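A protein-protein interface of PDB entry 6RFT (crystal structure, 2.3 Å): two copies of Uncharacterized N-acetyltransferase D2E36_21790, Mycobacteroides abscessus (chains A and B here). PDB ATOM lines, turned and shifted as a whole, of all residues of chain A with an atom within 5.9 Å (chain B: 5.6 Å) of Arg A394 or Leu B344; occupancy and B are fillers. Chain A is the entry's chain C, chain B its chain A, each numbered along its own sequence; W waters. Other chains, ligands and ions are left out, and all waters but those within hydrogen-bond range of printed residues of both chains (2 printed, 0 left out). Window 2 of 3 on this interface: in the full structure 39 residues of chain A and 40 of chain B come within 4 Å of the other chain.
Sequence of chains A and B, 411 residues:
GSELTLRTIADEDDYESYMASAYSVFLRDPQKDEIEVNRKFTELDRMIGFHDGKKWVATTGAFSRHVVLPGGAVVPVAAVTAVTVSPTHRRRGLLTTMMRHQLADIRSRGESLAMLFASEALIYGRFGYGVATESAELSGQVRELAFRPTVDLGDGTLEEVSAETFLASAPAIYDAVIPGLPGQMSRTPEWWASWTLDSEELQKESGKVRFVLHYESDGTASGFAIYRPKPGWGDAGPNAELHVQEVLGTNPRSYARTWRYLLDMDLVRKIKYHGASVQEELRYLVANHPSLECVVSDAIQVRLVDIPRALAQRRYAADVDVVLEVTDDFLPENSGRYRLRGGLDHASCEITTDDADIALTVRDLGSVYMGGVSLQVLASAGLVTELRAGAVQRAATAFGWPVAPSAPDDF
Of chain B, only Leu B344 comes within 4 Å of Arg A394. Leu B344 touches two residues of chain A. Printed residues of chain A within 4 Å of Ala B317: Thr A397. Of the printed residues of chain B, Gln A393 touches Leu B344 (3.7 Å) and Trp B401 (3.5 Å). Ala A396 touches none of the printed residues of chain B.
The backbone carbonyl oxygen (O) of Tyr B316 sits at hydrogen-bond distance from the backbone NH (N) of Leu B344. The backbone carbonyl oxygen (O) of Gly A390 is in hydrogen-bond range of the guanidinium group (NH1) of Arg A394, 3.0 Å away. The side-chain hydroxyl (OG1) of Thr A397 sits at hydrogen-bond distance from the backbone carbonyl oxygen (O) of Gln A393 (3.2 Å).
Along chain A the printed residues that touch a printed residue of chain B span positions 393 to 397. Of the 11 printed residues of chain B, 3 touch a printed residue of chain A. Printed residues of chain B that touch a printed residue of chain A: Ala B317, Leu B344 and Trp B401. Hydrophobic or aromatic side chains of chain B within 4 Å of the printed part of chain A: Ala B317, Leu B344 and Trp B401. Among the printed residues, 4 pairs touch across the chains. Among the printed residues, no Asp or Glu carboxylate lies within 4 Å of a Lys or Arg side-chain nitrogen of the other chain.
Water W1 lies within hydrogen-bond range of the backbone carbonyl oxygen (O) of Ala B317 (2.5 Å), the side-chain hydroxyl (OG1) of Thr A397 (2.5 Å) and the side-chain amide nitrogen (NE2) of Gln A393 (3.4 Å). Water W2 bridges the side-chain hydroxyl (OG1) of Thr A397 (3.1 Å) and the backbone NH (N) of Trp B401 (3.3 Å).
Position printed for both chains: 319. Of the 4 pairs that touch across the chains among the printed residues, none has its exchanged pair printed and touching as well.
Among the printed residues, pairs that only touch across the chains: Gln A393 with Leu B344, Gln A393 with Trp B401, Arg A394 with Leu B344 and Thr A397 with Ala B317.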
ATOM      1  N   ASP A 319     -11.365   4.879   4.204  1.00  0.00           N
ATOM      2  CA  ASP A 319     -12.734   5.189   4.593  1.00  0.00           C
ATOM      3  C   ASP A 319     -12.970   4.820   6.052  1.00  0.00           C
ATOM      4  O   ASP A 319     -12.447   3.818   6.549  1.00  0.00           O
ATOM      5  CB  ASP A 319     -13.726   4.453   3.690  1.00  0.00           C
ATOM      6  CG  ASP A 319     -13.805   5.055   2.300  1.00  0.00           C
ATOM      7  OD1 ASP A 319     -13.670   6.291   2.177  1.00  0.00           O
ATOM      8  OD2 ASP A 319     -14.006   4.293   1.330  1.00  0.00           O
ATOM      9  N   VAL A 320     -13.761   5.638   6.739  1.00  0.00           N
ATOM     10  CA  VAL A 320     -14.044   5.434   8.155  1.00  0.00           C
ATOM     11  C   VAL A 320     -15.434   5.970   8.460  1.00  0.00           C
ATOM     12  O   VAL A 320     -15.861   6.987   7.905  1.00  0.00           O
ATOM     13  CB  VAL A 320     -12.977   6.106   9.047  1.00  0.00           C
ATOM     14  CG1 VAL A 320     -12.934   7.611   8.800  1.00  0.00           C
ATOM     15  CG2 VAL A 320     -13.222   5.797  10.519  1.00  0.00           C
ATOM     16  N   ALA A 389     -16.604  -3.489  19.069  1.00  0.00           N
ATOM     17  CA  ALA A 389     -15.491  -4.236  18.498  1.00  0.00           C
ATOM     18  C   ALA A 389     -15.240  -3.834  17.050  1.00  0.00           C
ATOM     19  O   ALA A 389     -16.173  -3.591  16.281  1.00  0.00           O
ATOM     20  CB  ALA A 389     -15.769  -5.737  18.586  1.00  0.00           C
ATOM     21  N   GLY A 390     -13.959  -3.765  16.682  1.00  0.00           N
ATOM     22  CA  GLY A 390     -13.554  -3.437  15.332  1.00  0.00           C
ATOM     23  C   GLY A 390     -13.498  -1.961  15.007  1.00  0.00           C
ATOM     24  O   GLY A 390     -13.006  -1.602  13.929  1.00  0.00           O
ATOM     25  N   ALA A 391     -13.971  -1.089  15.900  1.00  0.00           N
ATOM     26  CA  ALA A 391     -14.014   0.335  15.587  1.00  0.00           C
ATOM     27  C   ALA A 391     -12.625   0.961  15.641  1.00  0.00           C
ATOM     28  O   ALA A 391     -12.260   1.750  14.761  1.00  0.00           O
ATOM     29  CB  ALA A 391     -14.965   1.054  16.542  1.00  0.00           C
ATOM     30  N   VAL A 392     -11.843   0.627  16.671  1.00  0.00           N
ATOM     31  CA  VAL A 392     -10.525   1.232  16.839  1.00  0.00           C
ATOM     32  C   VAL A 392      -9.617   0.868  15.670  1.00  0.00           C
ATOM     33  O   VAL A 392      -8.849   1.705  15.177  1.00  0.00           O
ATOM     34  CB  VAL A 392      -9.914   0.813  18.190  1.00  0.00           C
ATOM     35  CG1 VAL A 392      -8.436   1.171  18.249  1.00  0.00           C
ATOM     36  CG2 VAL A 392     -10.666   1.470  19.336  1.00  0.00           C
ATOM     37  N   GLN A 393      -9.693  -0.382  15.207  1.00  0.00           N
ATOM     38  CA  GLN A 393      -8.839  -0.836  14.111  1.00  0.00           C
ATOM     39  C   GLN A 393      -9.016   0.030  12.869  1.00  0.00           C
ATOM     40  O   GLN A 393      -8.037   0.527  12.299  1.00  0.00           O
ATOM     41  CB  GLN A 393      -9.150  -2.299  13.790  1.00  0.00           C
ATOM     42  CG  GLN A 393      -8.640  -2.766  12.434  1.00  0.00           C
ATOM     43  CD  GLN A 393      -7.346  -3.547  12.527  1.00  0.00           C
ATOM     44  OE1 GLN A 393      -7.071  -4.199  13.535  1.00  0.00           O
ATOM     45  NE2 GLN A 393      -6.542  -3.488  11.471  1.00  0.00           N
ATOM     46  N   ARG A 394     -10.263   0.222  12.432  1.00  0.00           N
ATOM     47  CA  ARG A 394     -10.510   1.012  11.230  1.00  0.00           C
ATOM     48  C   ARG A 394     -10.242   2.493  11.466  1.00  0.00           C
ATOM     49  O   ARG A 394      -9.728   3.184  10.579  1.00  0.00           O
ATOM     50  CB  ARG A 394     -11.940   0.787  10.741  1.00  0.00           C
ATOM     51  CG  ARG A 394     -12.177  -0.607  10.188  1.00  0.00           C
ATOM     52  CD  ARG A 394     -13.653  -0.966  10.169  1.00  0.00           C
ATOM     53  NE  ARG A 394     -13.878  -2.286   9.589  1.00  0.00           N
ATOM     54  CZ  ARG A 394     -13.748  -3.429  10.255  1.00  0.00           C
ATOM     55  NH1 ARG A 394     -13.388  -3.419  11.531  1.00  0.00           N
ATOM     56  NH2 ARG A 394     -13.974  -4.583   9.643  1.00  0.00           N
ATOM     57  N   ALA A 395     -10.580   3.000  12.654  1.00  0.00           N
ATOM     58  CA  ALA A 395     -10.317   4.404  12.955  1.00  0.00           C
ATOM     59  C   ALA A 395      -8.821   4.690  13.003  1.00  0.00           C
ATOM     60  O   ALA A 395      -8.373   5.751  12.550  1.00  0.00           O
ATOM     61  CB  ALA A 395     -10.983   4.793  14.274  1.00  0.00           C
ATOM     62  N   ALA A 396      -8.033   3.761  13.550  1.00  0.00           N
ATOM     63  CA  ALA A 396      -6.588   3.962  13.616  1.00  0.00           C
ATOM     64  C   ALA A 396      -5.980   4.053  12.222  1.00  0.00           C
ATOM     65  O   ALA A 396      -5.101   4.887  11.972  1.00  0.00           O
ATOM     66  CB  ALA A 396      -5.934   2.837  14.415  1.00  0.00           C
ATOM     67  N   THR A 397      -6.434   3.199  11.302  1.00  0.00           N
ATOM     68  CA  THR A 397      -5.923   3.245   9.935  1.00  0.00           C
ATOM     69  C   THR A 397      -6.317   4.543   9.242  1.00  0.00           C
ATOM     70  O   THR A 397      -5.506   5.143   8.527  1.00  0.00           O
ATOM     71  CB  THR A 397      -6.436   2.040   9.146  1.00  0.00           C
ATOM     72  OG1 THR A 397      -6.004   0.830   9.782  1.00  0.00           O
ATOM     73  CG2 THR A 397      -5.911   2.071   7.719  1.00  0.00           C
ATOM     74  N   ALA A 398      -7.556   4.995   9.446  1.00  0.00           N
ATOM     75  CA  ALA A 398      -8.012   6.227   8.811  1.00  0.00           C
ATOM     76  C   ALA A 398      -7.282   7.444   9.363  1.00  0.00           C
ATOM     77  O   ALA A 398      -6.885   8.333   8.602  1.00  0.00           O
ATOM     78  CB  ALA A 398      -9.517   6.381   8.991  1.00  0.00           C
ATOM     79  N   PHE A 399      -7.105   7.508  10.685  1.00  0.00           N
ATOM     80  CA  PHE A 399      -6.373   8.617  11.283  1.00  0.00           C
ATOM     81  C   PHE A 399      -4.896   8.614  10.913  1.00  0.00           C
ATOM     82  O   PHE A 399      -4.222   9.628  11.121  1.00  0.00           O
ATOM     83  CB  PHE A 399      -6.527   8.597  12.804  1.00  0.00           C
ATOM     84  CG  PHE A 399      -7.723   9.360  13.303  1.00  0.00           C
ATOM     85  CD1 PHE A 399      -7.660  10.733  13.474  1.00  0.00           C
ATOM     86  CD2 PHE A 399      -8.907   8.707  13.601  1.00  0.00           C
ATOM     87  CE1 PHE A 399      -8.755  11.442  13.933  1.00  0.00           C
ATOM     88  CE2 PHE A 399     -10.007   9.410  14.061  1.00  0.00           C
ATOM     89  CZ  PHE A 399      -9.930  10.779  14.227  1.00  0.00           C
ATOM     90  N   ARG B 315      -3.300 -10.014   6.090  1.00  0.00           N
ATOM     91  CA  ARG B 315      -4.440  -9.137   5.883  1.00  0.00           C
ATOM     92  C   ARG B 315      -3.966  -7.693   5.790  1.00  0.00           C
ATOM     93  O   ARG B 315      -2.854  -7.351   6.200  1.00  0.00           O
ATOM     94  CB  ARG B 315      -5.473  -9.288   7.007  1.00  0.00           C
ATOM     95  CG  ARG B 315      -6.279 -10.578   6.955  1.00  0.00           C
ATOM     96  CD  ARG B 315      -7.019 -10.659   5.625  1.00  0.00           C
ATOM     97  NE  ARG B 315      -7.819 -11.872   5.467  1.00  0.00           N
ATOM     98  CZ  ARG B 315      -7.402 -12.974   4.856  1.00  0.00           C
ATOM     99  NH1 ARG B 315      -6.182 -13.033   4.342  1.00  0.00           N
ATOM    100  NH2 ARG B 315      -8.212 -14.019   4.753  1.00  0.00           N
ATOM    101  N   TYR B 316      -4.829  -6.844   5.242  1.00  0.00           N
ATOM    102  CA  TYR B 316      -4.466  -5.475   4.908  1.00  0.00           C
ATOM    103  C   TYR B 316      -5.382  -4.494   5.623  1.00  0.00           C
ATOM    104  O   TYR B 316      -6.582  -4.744   5.777  1.00  0.00           O
ATOM    105  CB  TYR B 316      -4.516  -5.266   3.391  1.00  0.00           C
ATOM    106  CG  TYR B 316      -3.521  -6.138   2.657  1.00  0.00           C
ATOM    107  CD1 TYR B 316      -3.836  -7.445   2.305  1.00  0.00           C
ATOM    108  CD2 TYR B 316      -2.256  -5.661   2.336  1.00  0.00           C
ATOM    109  CE1 TYR B 316      -2.923  -8.249   1.646  1.00  0.00           C
ATOM    110  CE2 TYR B 316      -1.339  -6.455   1.674  1.00  0.00           C
ATOM    111  CZ  TYR B 316      -1.676  -7.747   1.332  1.00  0.00           C
ATOM    112  OH  TYR B 316      -0.761  -8.538   0.675  1.00  0.00           O
ATOM    113  N   ALA B 317      -4.799  -3.377   6.064  1.00  0.00           N
ATOM    114  CA  ALA B 317      -5.525  -2.404   6.872  1.00  0.00           C
ATOM    115  C   ALA B 317      -6.682  -1.759   6.121  1.00  0.00           C
ATOM    116  O   ALA B 317      -7.624  -1.276   6.758  1.00  0.00           O
ATOM    117  CB  ALA B 317      -4.565  -1.324   7.374  1.00  0.00           C
ATOM    118  N   ALA B 318      -6.638  -1.738   4.791  1.00  0.00           N
ATOM    119  CA  ALA B 318      -7.709  -1.155   3.999  1.00  0.00           C
ATOM    120  C   ALA B 318      -7.791  -1.881   2.665  1.00  0.00           C
ATOM    121  O   ALA B 318      -6.890  -2.631   2.286  1.00  0.00           O
ATOM    122  CB  ALA B 318      -7.497   0.347   3.789  1.00  0.00           C
ATOM    123  N   ASP B 319      -8.895  -1.649   1.955  1.00  0.00           N
ATOM    124  CA  ASP B 319      -9.094  -2.288   0.662  1.00  0.00           C
ATOM    125  C   ASP B 319      -8.041  -1.822  -0.333  1.00  0.00           C
ATOM    126  O   ASP B 319      -7.636  -0.656  -0.338  1.00  0.00           O
ATOM    127  CB  ASP B 319     -10.493  -1.980   0.125  1.00  0.00           C
ATOM    128  CG  ASP B 319     -11.581  -2.741   0.856  1.00  0.00           C
ATOM    129  OD1 ASP B 319     -11.331  -3.894   1.265  1.00  0.00           O
ATOM    130  OD2 ASP B 319     -12.688  -2.185   1.020  1.00  0.00           O
ATOM    131  N   GLY B 342      -6.704  -7.172  -1.615  1.00  0.00           N
ATOM    132  CA  GLY B 342      -6.659  -7.449  -0.196  1.00  0.00           C
ATOM    133  C   GLY B 342      -7.507  -6.474   0.594  1.00  0.00           C
ATOM    134  O   GLY B 342      -7.849  -5.382   0.132  1.00  0.00           O
ATOM    135  N   GLY B 343      -7.839  -6.898   1.802  1.00  0.00           N
ATOM    136  CA  GLY B 343      -8.612  -6.094   2.717  1.00  0.00           C
ATOM    137  C   GLY B 343      -8.467  -6.625   4.121  1.00  0.00           C
ATOM    138  O   GLY B 343      -7.522  -7.348   4.437  1.00  0.00           O
ATOM    139  N   LEU B 344      -9.426  -6.258   4.973  1.00  0.00           N
ATOM    140  CA  LEU B 344      -9.386  -6.717   6.356  1.00  0.00           C
ATOM    141  C   LEU B 344      -9.760  -8.189   6.483  1.00  0.00           C
ATOM    142  O   LEU B 344      -9.319  -8.856   7.426  1.00  0.00           O
ATOM    143  CB  LEU B 344     -10.304  -5.859   7.225  1.00  0.00           C
ATOM    144  CG  LEU B 344      -9.702  -4.538   7.711  1.00  0.00           C
ATOM    145  CD1 LEU B 344     -10.721  -3.741   8.509  1.00  0.00           C
ATOM    146  CD2 LEU B 344      -8.450  -4.794   8.537  1.00  0.00           C
ATOM    147  N   ASP B 345     -10.560  -8.721   5.550  1.00  0.00           N
ATOM    148  CA  ASP B 345     -11.048 -10.092   5.667  1.00  0.00           C
ATOM    149  C   ASP B 345     -10.824 -10.905   4.395  1.00  0.00           C
ATOM    150  O   ASP B 345     -11.458 -11.951   4.220  1.00  0.00           O
ATOM    151  CB  ASP B 345     -12.533 -10.110   6.042  1.00  0.00           C
ATOM    152  CG  ASP B 345     -13.396  -9.329   5.066  1.00  0.00           C
ATOM    153  OD1 ASP B 345     -12.841  -8.693   4.146  1.00  0.00           O
ATOM    154  OD2 ASP B 345     -14.635  -9.354   5.221  1.00  0.00           O
ATOM    155  N   HIS B 346      -9.940 -10.457   3.507  1.00  0.00           N
ATOM    156  CA  HIS B 346      -9.652 -11.206   2.292  1.00  0.00           C
ATOM    157  C   HIS B 346      -8.315 -10.742   1.738  1.00  0.00           C
ATOM    158  O   HIS B 346      -7.886  -9.611   1.980  1.00  0.00           O
ATOM    159  CB  HIS B 346     -10.756 -11.041   1.239  1.00  0.00           C
ATOM    160  CG  HIS B 346     -10.745  -9.713   0.546  1.00  0.00           C
ATOM    161  ND1 HIS B 346     -11.362  -8.596   1.066  1.00  0.00           N
ATOM    162  CD2 HIS B 346     -10.190  -9.326  -0.626  1.00  0.00           C
ATOM    163  CE1 HIS B 346     -11.188  -7.578   0.243  1.00  0.00           C
ATOM    164  NE2 HIS B 346     -10.480  -7.993  -0.792  1.00  0.00           N
ATOM    165  N   TRP B 401      -0.469  -1.215   9.002  1.00  0.00           N
ATOM    166  CA  TRP B 401      -1.220  -1.909  10.036  1.00  0.00           C
ATOM    167  C   TRP B 401      -1.303  -1.014  11.259  1.00  0.00           C
ATOM    168  O   TRP B 401      -0.323  -0.318  11.562  1.00  0.00           O
ATOM    169  CB  TRP B 401      -0.564  -3.248  10.395  1.00  0.00           C
ATOM    170  CG  TRP B 401      -1.444  -4.163  11.191  1.00  0.00           C
ATOM    171  CD1 TRP B 401      -1.306  -4.492  12.508  1.00  0.00           C
ATOM    172  CD2 TRP B 401      -2.611  -4.854  10.726  1.00  0.00           C
ATOM    173  NE1 TRP B 401      -2.307  -5.352  12.889  1.00  0.00           N
ATOM    174  CE2 TRP B 401      -3.123  -5.589  11.814  1.00  0.00           C
ATOM    175  CE3 TRP B 401      -3.270  -4.924   9.495  1.00  0.00           C
ATOM    176  CZ2 TRP B 401      -4.262  -6.384  11.708  1.00  0.00           C
ATOM    177  CZ3 TRP B 401      -4.402  -5.714   9.392  1.00  0.00           C
ATOM    178  CH2 TRP B 401      -4.886  -6.433  10.492  1.00  0.00           C
HETATM  179  O   HOH W   1      -7.532  -1.099   9.204  1.00  0.00           O
HETATM  180  O   HOH W   2      -2.919   0.987   9.348  1.00  0.00           O
